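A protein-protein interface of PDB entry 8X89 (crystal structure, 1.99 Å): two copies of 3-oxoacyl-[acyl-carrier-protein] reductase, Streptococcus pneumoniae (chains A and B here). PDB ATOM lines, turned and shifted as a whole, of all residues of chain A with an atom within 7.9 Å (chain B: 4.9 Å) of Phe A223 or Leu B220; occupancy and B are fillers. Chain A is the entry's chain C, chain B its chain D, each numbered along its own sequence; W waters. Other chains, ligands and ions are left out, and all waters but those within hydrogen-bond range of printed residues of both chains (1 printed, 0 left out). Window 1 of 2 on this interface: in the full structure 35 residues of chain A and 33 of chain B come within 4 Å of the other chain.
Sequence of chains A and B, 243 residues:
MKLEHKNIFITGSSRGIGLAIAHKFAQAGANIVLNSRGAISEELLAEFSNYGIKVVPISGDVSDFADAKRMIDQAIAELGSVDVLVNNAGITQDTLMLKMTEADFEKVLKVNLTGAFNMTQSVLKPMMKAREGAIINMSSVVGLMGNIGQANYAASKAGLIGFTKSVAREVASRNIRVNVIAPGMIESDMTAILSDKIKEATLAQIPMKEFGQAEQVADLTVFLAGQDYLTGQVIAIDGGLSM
Of the 12 printed residues of chain B, 6 touch a printed residue of chain A.
Hydrophobic or aromatic side chains of chain B within 4 Å of the printed part of chain A: Leu B220, Phe B223 and Ile B237.
Printed residues of chain A that touch a printed residue of chain B: Lys A2, Asp A219, Leu A220, Phe A223, Gln A227, Asp A228 and Gln A233.
Among the printed residues, 12 pairs touch across the chains.
Among the printed residues, Asp or Glu carboxylates within 4 Å of a Lys or Arg side-chain nitrogen of the other chain: Lys A2 with Asp B219 (3.2 Å).
The backbone carbonyl oxygen of Gly A226 lies close to the side-chain amino group of Lys A2 (3.3 Å).
The side-chain amino group of Lys A2 is in hydrogen-bond range of the side-chain amide oxygen of Gln A227, 3.4 Å away.
The side-chain amino group (NZ) of Lys A24 lies within salt-bridge range of the side-chain carboxylate (OD2) of Asp A219 (3.3 Å).
The guanidinium group of Arg A177 is in hydrogen-bond range of the backbone carbonyl oxygen of Gln A227, at 2.8 Å.
Water W1 lies within hydrogen-bond range of OD2 of Asp B219, NE2 of Gln A227 and NZ of Lys A2.
NZ of Lys A2 is in salt-bridge range of OD2 of Asp B219, 3.2 Å away.
Phe A223 touches just these residues of chain B: Asp B219 (3.9 Å), Leu B220 (3.6 Å) and Phe B223 (3.6 Å).
Of chain A, only Phe A223 comes within 4 Å of Leu B220.
Printed residues of chain B within 4 Å of Leu A220: Phe B223.
Printed residues of chain B within 4 Å of Gln A227: Gln B216, Asp B219 and Ile B237.
Of the printed residues of chain B, Gln A233 touches Ile B235.
Of the printed residues of chain B, Lys A2 touches Asp B219 (3.2 Å).
The nearest printed residue of chain B that does not touch Phe A223 is Gln B216 (5.7 Å).
The nearest printed residue of chain A that does not touch Asp B219 is Gly A226 (6.4 Å).
Among the printed residues, merely in contact across the chains: Asp A219 with Phe B223, Leu A220 with Phe B223, Phe A223 with Asp B219, Phe A223 with Leu B220, Phe A223 with Phe B223, Gln A227 with Gln B216, Gln A227 with Asp B219, Gln A227 with Ile B237, Asp A228 with Gln B216, Asp A228 with Ile B237 and Gln A233 with Ile B235.
Asp A219 touches Phe B223, and with the chains exchanged Phe A223 touches Asp B219.
Leu A220 touches Phe B223, and with the chains exchanged Phe A223 touches Leu B220.
Phe A223 touches its own counterpart, Phe B223.
10 positions are printed for both chains.
Of the 12 pairs that touch across the chains among the printed residues, 5 have their exchanged pair printed and touching as well.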
ATOM      1  N   LYS A   2     -18.466  11.270 -21.199  1.00  0.00           N
ATOM      2  CA  LYS A   2     -19.029  11.490 -22.519  1.00  0.00           C
ATOM      3  C   LYS A   2     -20.477  11.033 -22.610  1.00  0.00           C
ATOM      4  O   LYS A   2     -21.103  11.215 -23.656  1.00  0.00           O
ATOM      5  CB  LYS A   2     -18.179  10.756 -23.564  1.00  0.00           C
ATOM      6  CG  LYS A   2     -16.705  11.164 -23.529  1.00  0.00           C
ATOM      7  CD  LYS A   2     -15.967  10.850 -24.823  1.00  0.00           C
ATOM      8  CE  LYS A   2     -15.522   9.399 -24.873  1.00  0.00           C
ATOM      9  NZ  LYS A   2     -14.528   9.154 -25.963  1.00  0.00           N
ATOM     10  N   LEU A   3     -21.032  10.453 -21.542  1.00  0.00           N
ATOM     11  CA  LEU A   3     -22.297   9.745 -21.655  1.00  0.00           C
ATOM     12  C   LEU A   3     -23.373  10.216 -20.677  1.00  0.00           C
ATOM     13  O   LEU A   3     -24.504   9.709 -20.740  1.00  0.00           O
ATOM     14  CB  LEU A   3     -22.054   8.237 -21.468  1.00  0.00           C
ATOM     15  CG  LEU A   3     -21.301   7.458 -22.560  1.00  0.00           C
ATOM     16  CD1 LEU A   3     -21.152   6.005 -22.134  1.00  0.00           C
ATOM     17  CD2 LEU A   3     -21.987   7.529 -23.918  1.00  0.00           C
ATOM     18  N   LYS A  24     -22.541  -0.677 -16.117  1.00  0.00           N
ATOM     19  CA  LYS A  24     -21.487   0.222 -16.596  1.00  0.00           C
ATOM     20  C   LYS A  24     -22.073   1.503 -17.178  1.00  0.00           C
ATOM     21  O   LYS A  24     -21.531   2.595 -16.963  1.00  0.00           O
ATOM     22  CB  LYS A  24     -20.618  -0.462 -17.664  1.00  0.00           C
ATOM     23  CG  LYS A  24     -19.685  -1.474 -17.135  1.00  0.00           C
ATOM     24  CD  LYS A  24     -18.595  -0.871 -16.292  1.00  0.00           C
ATOM     25  CE  LYS A  24     -17.743  -2.014 -15.736  1.00  0.00           C
ATOM     26  NZ  LYS A  24     -16.667  -1.591 -14.788  1.00  0.00           N
ATOM     27  N   PHE A  25     -23.143   1.390 -17.962  1.00  0.00           N
ATOM     28  CA  PHE A  25     -23.772   2.616 -18.461  1.00  0.00           C
ATOM     29  C   PHE A  25     -24.294   3.477 -17.315  1.00  0.00           C
ATOM     30  O   PHE A  25     -24.125   4.704 -17.328  1.00  0.00           O
ATOM     31  CB  PHE A  25     -24.882   2.288 -19.447  1.00  0.00           C
ATOM     32  CG  PHE A  25     -24.390   2.115 -20.869  1.00  0.00           C
ATOM     33  CD1 PHE A  25     -23.797   3.183 -21.548  1.00  0.00           C
ATOM     34  CD2 PHE A  25     -24.529   0.890 -21.528  1.00  0.00           C
ATOM     35  CE1 PHE A  25     -23.339   3.035 -22.876  1.00  0.00           C
ATOM     36  CE2 PHE A  25     -24.075   0.727 -22.877  1.00  0.00           C
ATOM     37  CZ  PHE A  25     -23.469   1.802 -23.535  1.00  0.00           C
ATOM     38  N   ILE A 136     -24.566  -0.909 -31.178  1.00  0.00           N
ATOM     39  CA  ILE A 136     -23.551  -1.874 -30.798  1.00  0.00           C
ATOM     40  C   ILE A 136     -24.207  -3.233 -30.836  1.00  0.00           C
ATOM     41  O   ILE A 136     -25.097  -3.531 -30.018  1.00  0.00           O
ATOM     42  CB  ILE A 136     -22.972  -1.567 -29.421  1.00  0.00           C
ATOM     43  CG1 ILE A 136     -22.331  -0.183 -29.492  1.00  0.00           C
ATOM     44  CG2 ILE A 136     -21.920  -2.651 -29.024  1.00  0.00           C
ATOM     45  CD1 ILE A 136     -21.997   0.436 -28.209  1.00  0.00           C
ATOM     46  N   ARG A 177     -22.647   5.549 -35.733  1.00  0.00           N
ATOM     47  CA  ARG A 177     -21.586   4.554 -35.613  1.00  0.00           C
ATOM     48  C   ARG A 177     -22.198   3.195 -35.315  1.00  0.00           C
ATOM     49  O   ARG A 177     -23.030   3.071 -34.410  1.00  0.00           O
ATOM     50  CB  ARG A 177     -20.620   4.949 -34.511  1.00  0.00           C
ATOM     51  CG  ARG A 177     -19.954   6.284 -34.756  1.00  0.00           C
ATOM     52  CD  ARG A 177     -19.373   6.829 -33.465  1.00  0.00           C
ATOM     53  NE  ARG A 177     -20.370   7.603 -32.739  1.00  0.00           N
ATOM     54  CZ  ARG A 177     -20.656   7.458 -31.446  1.00  0.00           C
ATOM     55  NH1 ARG A 177     -20.004   6.582 -30.693  1.00  0.00           N
ATOM     56  NH2 ARG A 177     -21.597   8.212 -30.898  1.00  0.00           N
ATOM     57  N   ILE A 181     -19.374  -6.381 -31.310  1.00  0.00           N
ATOM     58  CA  ILE A 181     -18.458  -7.011 -30.374  1.00  0.00           C
ATOM     59  C   ILE A 181     -18.634  -8.517 -30.476  1.00  0.00           C
ATOM     60  O   ILE A 181     -19.763  -9.013 -30.432  1.00  0.00           O
ATOM     61  CB  ILE A 181     -18.703  -6.529 -28.940  1.00  0.00           C
ATOM     62  CG1 ILE A 181     -18.362  -5.033 -28.876  1.00  0.00           C
ATOM     63  CG2 ILE A 181     -17.883  -7.406 -27.942  1.00  0.00           C
ATOM     64  CD1 ILE A 181     -18.790  -4.356 -27.604  1.00  0.00           C
ATOM     65  N   VAL A 217     -16.592  -7.281 -21.455  1.00  0.00           N
ATOM     66  CA  VAL A 217     -17.534  -6.981 -22.529  1.00  0.00           C
ATOM     67  C   VAL A 217     -18.250  -5.662 -22.254  1.00  0.00           C
ATOM     68  O   VAL A 217     -18.442  -4.839 -23.159  1.00  0.00           O
ATOM     69  CB  VAL A 217     -18.536  -8.137 -22.696  1.00  0.00           C
ATOM     70  CG1 VAL A 217     -19.527  -7.827 -23.822  1.00  0.00           C
ATOM     71  CG2 VAL A 217     -17.798  -9.489 -22.909  1.00  0.00           C
ATOM     72  N   ALA A 218     -18.659  -5.439 -21.002  1.00  0.00           N
ATOM     73  CA  ALA A 218     -19.388  -4.216 -20.669  1.00  0.00           C
ATOM     74  C   ALA A 218     -18.520  -2.964 -20.852  1.00  0.00           C
ATOM     75  O   ALA A 218     -19.001  -1.939 -21.367  1.00  0.00           O
ATOM     76  CB  ALA A 218     -19.903  -4.308 -19.233  1.00  0.00           C
ATOM     77  N   ASP A 219     -17.248  -3.023 -20.433  1.00  0.00           N
ATOM     78  CA  ASP A 219     -16.346  -1.878 -20.611  1.00  0.00           C
ATOM     79  C   ASP A 219     -16.162  -1.533 -22.080  1.00  0.00           C
ATOM     80  O   ASP A 219     -16.093  -0.355 -22.445  1.00  0.00           O
ATOM     81  CB  ASP A 219     -14.980  -2.145 -19.988  1.00  0.00           C
ATOM     82  CG  ASP A 219     -14.996  -2.047 -18.462  1.00  0.00           C
ATOM     83  OD1 ASP A 219     -14.204  -2.742 -17.800  1.00  0.00           O
ATOM     84  OD2 ASP A 219     -15.795  -1.242 -17.935  1.00  0.00           O
ATOM     85  N   LEU A 220     -16.037  -2.553 -22.926  1.00  0.00           N
ATOM     86  CA  LEU A 220     -15.905  -2.325 -24.352  1.00  0.00           C
ATOM     87  C   LEU A 220     -17.182  -1.715 -24.935  1.00  0.00           C
ATOM     88  O   LEU A 220     -17.109  -0.806 -25.775  1.00  0.00           O
ATOM     89  CB  LEU A 220     -15.559  -3.641 -25.044  1.00  0.00           C
ATOM     90  CG  LEU A 220     -15.464  -3.514 -26.574  1.00  0.00           C
ATOM     91  CD1 LEU A 220     -14.352  -2.536 -26.958  1.00  0.00           C
ATOM     92  CD2 LEU A 220     -15.181  -4.869 -27.167  1.00  0.00           C
ATOM     93  N   THR A 221     -18.354  -2.221 -24.519  1.00  0.00           N
ATOM     94  CA  THR A 221     -19.625  -1.681 -25.011  1.00  0.00           C
ATOM     95  C   THR A 221     -19.779  -0.201 -24.659  1.00  0.00           C
ATOM     96  O   THR A 221     -20.169   0.609 -25.506  1.00  0.00           O
ATOM     97  CB  THR A 221     -20.791  -2.508 -24.457  1.00  0.00           C
ATOM     98  OG1 THR A 221     -20.606  -3.884 -24.840  1.00  0.00           O
ATOM     99  CG2 THR A 221     -22.152  -2.003 -24.989  1.00  0.00           C
ATOM    100  N   VAL A 222     -19.463   0.175 -23.421  1.00  0.00           N
ATOM    101  CA  VAL A 222     -19.578   1.577 -23.023  1.00  0.00           C
ATOM    102  C   VAL A 222     -18.587   2.433 -23.798  1.00  0.00           C
ATOM    103  O   VAL A 222     -18.900   3.563 -24.219  1.00  0.00           O
ATOM    104  CB  VAL A 222     -19.380   1.718 -21.504  1.00  0.00           C
ATOM    105  CG1 VAL A 222     -19.049   3.153 -21.127  1.00  0.00           C
ATOM    106  CG2 VAL A 222     -20.625   1.233 -20.760  1.00  0.00           C
ATOM    107  N   PHE A 223     -17.370   1.924 -23.992  1.00  0.00           N
ATOM    108  CA  PHE A 223     -16.363   2.717 -24.686  1.00  0.00           C
ATOM    109  C   PHE A 223     -16.803   3.031 -26.107  1.00  0.00           C
ATOM    110  O   PHE A 223     -16.776   4.194 -26.531  1.00  0.00           O
ATOM    111  CB  PHE A 223     -15.017   1.998 -24.711  1.00  0.00           C
ATOM    112  CG  PHE A 223     -14.022   2.659 -25.639  1.00  0.00           C
ATOM    113  CD1 PHE A 223     -13.389   3.846 -25.264  1.00  0.00           C
ATOM    114  CD2 PHE A 223     -13.782   2.141 -26.907  1.00  0.00           C
ATOM    115  CE1 PHE A 223     -12.467   4.478 -26.133  1.00  0.00           C
ATOM    116  CE2 PHE A 223     -12.872   2.766 -27.779  1.00  0.00           C
ATOM    117  CZ  PHE A 223     -12.217   3.928 -27.390  1.00  0.00           C
ATOM    118  N   LEU A 224     -17.232   2.006 -26.854  1.00  0.00           N
ATOM    119  CA  LEU A 224     -17.698   2.221 -28.225  1.00  0.00           C
ATOM    120  C   LEU A 224     -18.877   3.180 -28.265  1.00  0.00           C
ATOM    121  O   LEU A 224     -18.975   4.021 -29.173  1.00  0.00           O
ATOM    122  CB  LEU A 224     -18.112   0.900 -28.876  1.00  0.00           C
ATOM    123  CG  LEU A 224     -17.055  -0.162 -29.156  1.00  0.00           C
ATOM    124  CD1 LEU A 224     -17.755  -1.379 -29.739  1.00  0.00           C
ATOM    125  CD2 LEU A 224     -15.970   0.363 -30.080  1.00  0.00           C
ATOM    126  N   ALA A 225     -19.809   3.046 -27.309  1.00  0.00           N
ATOM    127  CA  ALA A 225     -20.972   3.925 -27.300  1.00  0.00           C
ATOM    128  C   ALA A 225     -20.556   5.386 -27.214  1.00  0.00           C
ATOM    129  O   ALA A 225     -21.215   6.246 -27.797  1.00  0.00           O
ATOM    130  CB  ALA A 225     -21.899   3.574 -26.132  1.00  0.00           C
ATOM    131  N   GLY A 226     -19.466   5.681 -26.512  1.00  0.00           N
ATOM    132  CA  GLY A 226     -19.019   7.044 -26.311  1.00  0.00           C
ATOM    133  C   GLY A 226     -17.936   7.534 -27.248  1.00  0.00           C
ATOM    134  O   GLY A 226     -17.562   8.710 -27.177  1.00  0.00           O
ATOM    135  N   GLN A 227     -17.418   6.674 -28.127  1.00  0.00           N
ATOM    136  CA  GLN A 227     -16.232   6.978 -28.919  1.00  0.00           C
ATOM    137  C   GLN A 227     -16.629   7.476 -30.307  1.00  0.00           C
ATOM    138  O   GLN A 227     -17.236   6.735 -31.090  1.00  0.00           O
ATOM    139  CB  GLN A 227     -15.328   5.748 -29.026  1.00  0.00           C
ATOM    140  CG  GLN A 227     -14.095   5.992 -29.837  1.00  0.00           C
ATOM    141  CD  GLN A 227     -13.345   7.192 -29.353  1.00  0.00           C
ATOM    142  OE1 GLN A 227     -12.918   7.250 -28.206  1.00  0.00           O
ATOM    143  NE2 GLN A 227     -13.202   8.186 -30.226  1.00  0.00           N
ATOM    144  N   ASP A 228     -16.284   8.727 -30.603  1.00  0.00           N
ATOM    145  CA  ASP A 228     -16.507   9.272 -31.936  1.00  0.00           C
ATOM    146  C   ASP A 228     -15.601   8.626 -32.984  1.00  0.00           C
ATOM    147  O   ASP A 228     -14.466   8.242 -32.704  1.00  0.00           O
ATOM    148  CB  ASP A 228     -16.267  10.780 -31.952  1.00  0.00           C
ATOM    149  CG  ASP A 228     -17.450  11.559 -31.438  1.00  0.00           C
ATOM    150  OD1 ASP A 228     -18.554  11.392 -31.997  1.00  0.00           O
ATOM    151  OD2 ASP A 228     -17.271  12.354 -30.491  1.00  0.00           O
ATOM    152  N   LEU A 230     -15.559   6.086 -34.861  1.00  0.00           N
ATOM    153  CA  LEU A 230     -15.222   4.667 -34.913  1.00  0.00           C
ATOM    154  C   LEU A 230     -16.459   3.884 -35.352  1.00  0.00           C
ATOM    155  O   LEU A 230     -17.422   3.754 -34.588  1.00  0.00           O
ATOM    156  CB  LEU A 230     -14.689   4.210 -33.545  1.00  0.00           C
ATOM    157  CG  LEU A 230     -13.957   2.879 -33.420  1.00  0.00           C
ATOM    158  CD1 LEU A 230     -13.227   2.785 -32.085  1.00  0.00           C
ATOM    159  CD2 LEU A 230     -14.962   1.729 -33.522  1.00  0.00           C
ATOM    160  N   GLN A 233     -16.478  -1.554 -37.292  1.00  0.00           N
ATOM    161  CA  GLN A 233     -15.478  -2.449 -36.724  1.00  0.00           C
ATOM    162  C   GLN A 233     -16.078  -3.736 -36.164  1.00  0.00           C
ATOM    163  O   GLN A 233     -17.203  -3.767 -35.649  1.00  0.00           O
ATOM    164  CB  GLN A 233     -14.702  -1.755 -35.612  1.00  0.00           C
ATOM    165  CG  GLN A 233     -14.028  -0.465 -36.006  1.00  0.00           C
ATOM    166  CD  GLN A 233     -13.070  -0.650 -37.169  1.00  0.00           C
ATOM    167  OE1 GLN A 233     -11.974  -1.164 -36.989  1.00  0.00           O
ATOM    168  NE2 GLN A 233     -13.487  -0.218 -38.375  1.00  0.00           N
ATOM    169  N   ILE A 235     -14.849  -6.215 -33.317  1.00  0.00           N
ATOM    170  CA  ILE A 235     -13.854  -6.207 -32.252  1.00  0.00           C
ATOM    171  C   ILE A 235     -14.054  -7.453 -31.416  1.00  0.00           C
ATOM    172  O   ILE A 235     -15.071  -7.601 -30.721  1.00  0.00           O
ATOM    173  CB  ILE A 235     -13.936  -4.933 -31.406  1.00  0.00           C
ATOM    174  CG1 ILE A 235     -13.877  -3.720 -32.344  1.00  0.00           C
ATOM    175  CG2 ILE A 235     -12.804  -4.898 -30.354  1.00  0.00           C
ATOM    176  CD1 ILE A 235     -13.650  -2.409 -31.659  1.00  0.00           C
ATOM    177  N   ILE B 181      -3.691   0.450 -33.675  1.00  0.00           N
ATOM    178  CA  ILE B 181      -4.676   1.470 -34.030  1.00  0.00           C
ATOM    179  C   ILE B 181      -4.371   1.966 -35.436  1.00  0.00           C
ATOM    180  O   ILE B 181      -3.215   2.268 -35.751  1.00  0.00           O
ATOM    181  CB  ILE B 181      -4.660   2.642 -33.031  1.00  0.00           C
ATOM    182  CG1 ILE B 181      -5.060   2.174 -31.635  1.00  0.00           C
ATOM    183  CG2 ILE B 181      -5.548   3.788 -33.524  1.00  0.00           C
ATOM    184  CD1 ILE B 181      -4.640   3.134 -30.557  1.00  0.00           C
ATOM    185  N   GLN B 216      -9.401  11.590 -30.338  1.00  0.00           N
ATOM    186  CA  GLN B 216     -10.038  10.287 -30.523  1.00  0.00           C
ATOM    187  C   GLN B 216      -9.007   9.159 -30.523  1.00  0.00           C
ATOM    188  O   GLN B 216      -9.229   8.108 -29.907  1.00  0.00           O
ATOM    189  CB  GLN B 216     -10.844  10.295 -31.817  1.00  0.00           C
ATOM    190  CG  GLN B 216     -11.925  11.359 -31.822  1.00  0.00           C
ATOM    191  CD  GLN B 216     -12.286  11.827 -33.227  1.00  0.00           C
ATOM    192  OE1 GLN B 216     -11.695  11.389 -34.222  1.00  0.00           O
ATOM    193  NE2 GLN B 216     -13.249  12.740 -33.309  1.00  0.00           N
ATOM    194  N   VAL B 217      -7.876   9.367 -31.204  1.00  0.00           N
ATOM    195  CA  VAL B 217      -6.781   8.399 -31.177  1.00  0.00           C
ATOM    196  C   VAL B 217      -6.240   8.230 -29.760  1.00  0.00           C
ATOM    197  O   VAL B 217      -5.973   7.105 -29.311  1.00  0.00           O
ATOM    198  CB  VAL B 217      -5.664   8.827 -32.156  1.00  0.00           C
ATOM    199  CG1 VAL B 217      -4.472   7.892 -32.043  1.00  0.00           C
ATOM    200  CG2 VAL B 217      -6.183   8.852 -33.586  1.00  0.00           C
ATOM    201  N   ALA B 218      -6.053   9.342 -29.038  1.00  0.00           N
ATOM    202  CA  ALA B 218      -5.517   9.254 -27.685  1.00  0.00           C
ATOM    203  C   ALA B 218      -6.470   8.498 -26.761  1.00  0.00           C
ATOM    204  O   ALA B 218      -6.025   7.703 -25.926  1.00  0.00           O
ATOM    205  CB  ALA B 218      -5.215  10.653 -27.145  1.00  0.00           C
ATOM    206  N   ASP B 219      -7.785   8.708 -26.926  1.00  0.00           N
ATOM    207  CA  ASP B 219      -8.792   8.017 -26.117  1.00  0.00           C
ATOM    208  C   ASP B 219      -8.781   6.513 -26.384  1.00  0.00           C
ATOM    209  O   ASP B 219      -8.848   5.700 -25.453  1.00  0.00           O
ATOM    210  CB  ASP B 219     -10.188   8.580 -26.422  1.00  0.00           C
ATOM    211  CG  ASP B 219     -10.516   9.820 -25.594  1.00  0.00           C
ATOM    212  OD1 ASP B 219      -9.694  10.193 -24.729  1.00  0.00           O
ATOM    213  OD2 ASP B 219     -11.580  10.444 -25.832  1.00  0.00           O
ATOM    214  N   LEU B 220      -8.754   6.129 -27.667  1.00  0.00           N
ATOM    215  CA  LEU B 220      -8.642   4.717 -28.016  1.00  0.00           C
ATOM    216  C   LEU B 220      -7.366   4.105 -27.434  1.00  0.00           C
ATOM    217  O   LEU B 220      -7.396   2.995 -26.888  1.00  0.00           O
ATOM    218  CB  LEU B 220      -8.694   4.552 -29.537  1.00  0.00           C
ATOM    219  CG  LEU B 220      -8.613   3.119 -30.063  1.00  0.00           C
ATOM    220  CD1 LEU B 220      -9.693   2.232 -29.409  1.00  0.00           C
ATOM    221  CD2 LEU B 220      -8.750   3.138 -31.589  1.00  0.00           C
ATOM    222  N   THR B 221      -6.242   4.824 -27.507  1.00  0.00           N
ATOM    223  CA  THR B 221      -4.992   4.302 -26.956  1.00  0.00           C
ATOM    224  C   THR B 221      -5.121   4.022 -25.457  1.00  0.00           C
ATOM    225  O   THR B 221      -4.714   2.955 -24.972  1.00  0.00           O
ATOM    226  CB  THR B 221      -3.835   5.279 -27.213  1.00  0.00           C
ATOM    227  OG1 THR B 221      -3.667   5.495 -28.625  1.00  0.00           O
ATOM    228  CG2 THR B 221      -2.555   4.731 -26.643  1.00  0.00           C
ATOM    229  N   VAL B 222      -5.683   4.972 -24.706  1.00  0.00           N
ATOM    230  CA  VAL B 222      -5.824   4.781 -23.257  1.00  0.00           C
ATOM    231  C   VAL B 222      -6.743   3.601 -22.960  1.00  0.00           C
ATOM    232  O   VAL B 222      -6.477   2.800 -22.049  1.00  0.00           O
ATOM    233  CB  VAL B 222      -6.319   6.080 -22.588  1.00  0.00           C
ATOM    234  CG1 VAL B 222      -6.833   5.799 -21.171  1.00  0.00           C
ATOM    235  CG2 VAL B 222      -5.194   7.094 -22.521  1.00  0.00           C
ATOM    236  N   PHE B 223      -7.820   3.458 -23.738  1.00  0.00           N
ATOM    237  CA  PHE B 223      -8.764   2.364 -23.518  1.00  0.00           C
ATOM    238  C   PHE B 223      -8.097   1.009 -23.721  1.00  0.00           C
ATOM    239  O   PHE B 223      -8.259   0.098 -22.908  1.00  0.00           O
ATOM    240  CB  PHE B 223      -9.970   2.481 -24.458  1.00  0.00           C
ATOM    241  CG  PHE B 223     -10.867   1.258 -24.413  1.00  0.00           C
ATOM    242  CD1 PHE B 223     -11.623   0.989 -23.284  1.00  0.00           C
ATOM    243  CD2 PHE B 223     -10.894   0.350 -25.466  1.00  0.00           C
ATOM    244  CE1 PHE B 223     -12.428  -0.159 -23.209  1.00  0.00           C
ATOM    245  CE2 PHE B 223     -11.683  -0.795 -25.402  1.00  0.00           C
ATOM    246  CZ  PHE B 223     -12.458  -1.051 -24.272  1.00  0.00           C
ATOM    247  N   LEU B 224      -7.385   0.842 -24.834  1.00  0.00           N
ATOM    248  CA  LEU B 224      -6.716  -0.429 -25.093  1.00  0.00           C
ATOM    249  C   LEU B 224      -5.716  -0.755 -23.991  1.00  0.00           C
ATOM    250  O   LEU B 224      -5.695  -1.883 -23.487  1.00  0.00           O
ATOM    251  CB  LEU B 224      -6.040  -0.417 -26.472  1.00  0.00           C
ATOM    252  CG  LEU B 224      -7.000  -0.255 -27.662  1.00  0.00           C
ATOM    253  CD1 LEU B 224      -6.282  -0.267 -29.010  1.00  0.00           C
ATOM    254  CD2 LEU B 224      -8.027  -1.364 -27.642  1.00  0.00           C
ATOM    255  N   ILE B 235      -7.761  -1.910 -34.965  1.00  0.00           N
ATOM    256  CA  ILE B 235      -8.923  -1.085 -34.692  1.00  0.00           C
ATOM    257  C   ILE B 235      -8.751   0.212 -35.449  1.00  0.00           C
ATOM    258  O   ILE B 235      -7.868   1.015 -35.128  1.00  0.00           O
ATOM    259  CB  ILE B 235      -9.122  -0.847 -33.191  1.00  0.00           C
ATOM    260  CG1 ILE B 235      -9.324  -2.214 -32.509  1.00  0.00           C
ATOM    261  CG2 ILE B 235     -10.333   0.044 -32.981  1.00  0.00           C
ATOM    262  CD1 ILE B 235      -9.429  -2.183 -31.025  1.00  0.00           C
ATOM    263  N   ILE B 237      -9.800   3.813 -36.331  1.00  0.00           N
ATOM    264  CA  ILE B 237     -10.610   4.946 -35.920  1.00  0.00           C
ATOM    265  C   ILE B 237     -10.462   6.020 -37.002  1.00  0.00           C
ATOM    266  O   ILE B 237      -9.697   6.984 -36.872  1.00  0.00           O
ATOM    267  CB  ILE B 237     -10.245   5.403 -34.489  1.00  0.00           C
ATOM    268  CG1 ILE B 237     -11.211   6.495 -33.997  1.00  0.00           C
ATOM    269  CG2 ILE B 237      -8.736   5.697 -34.325  1.00  0.00           C
ATOM    270  CD1 ILE B 237     -11.146   6.727 -32.494  1.00  0.00           C
HETATM  271  O   HOH W   1     -12.511  10.778 -28.290  1.00  0.00           O
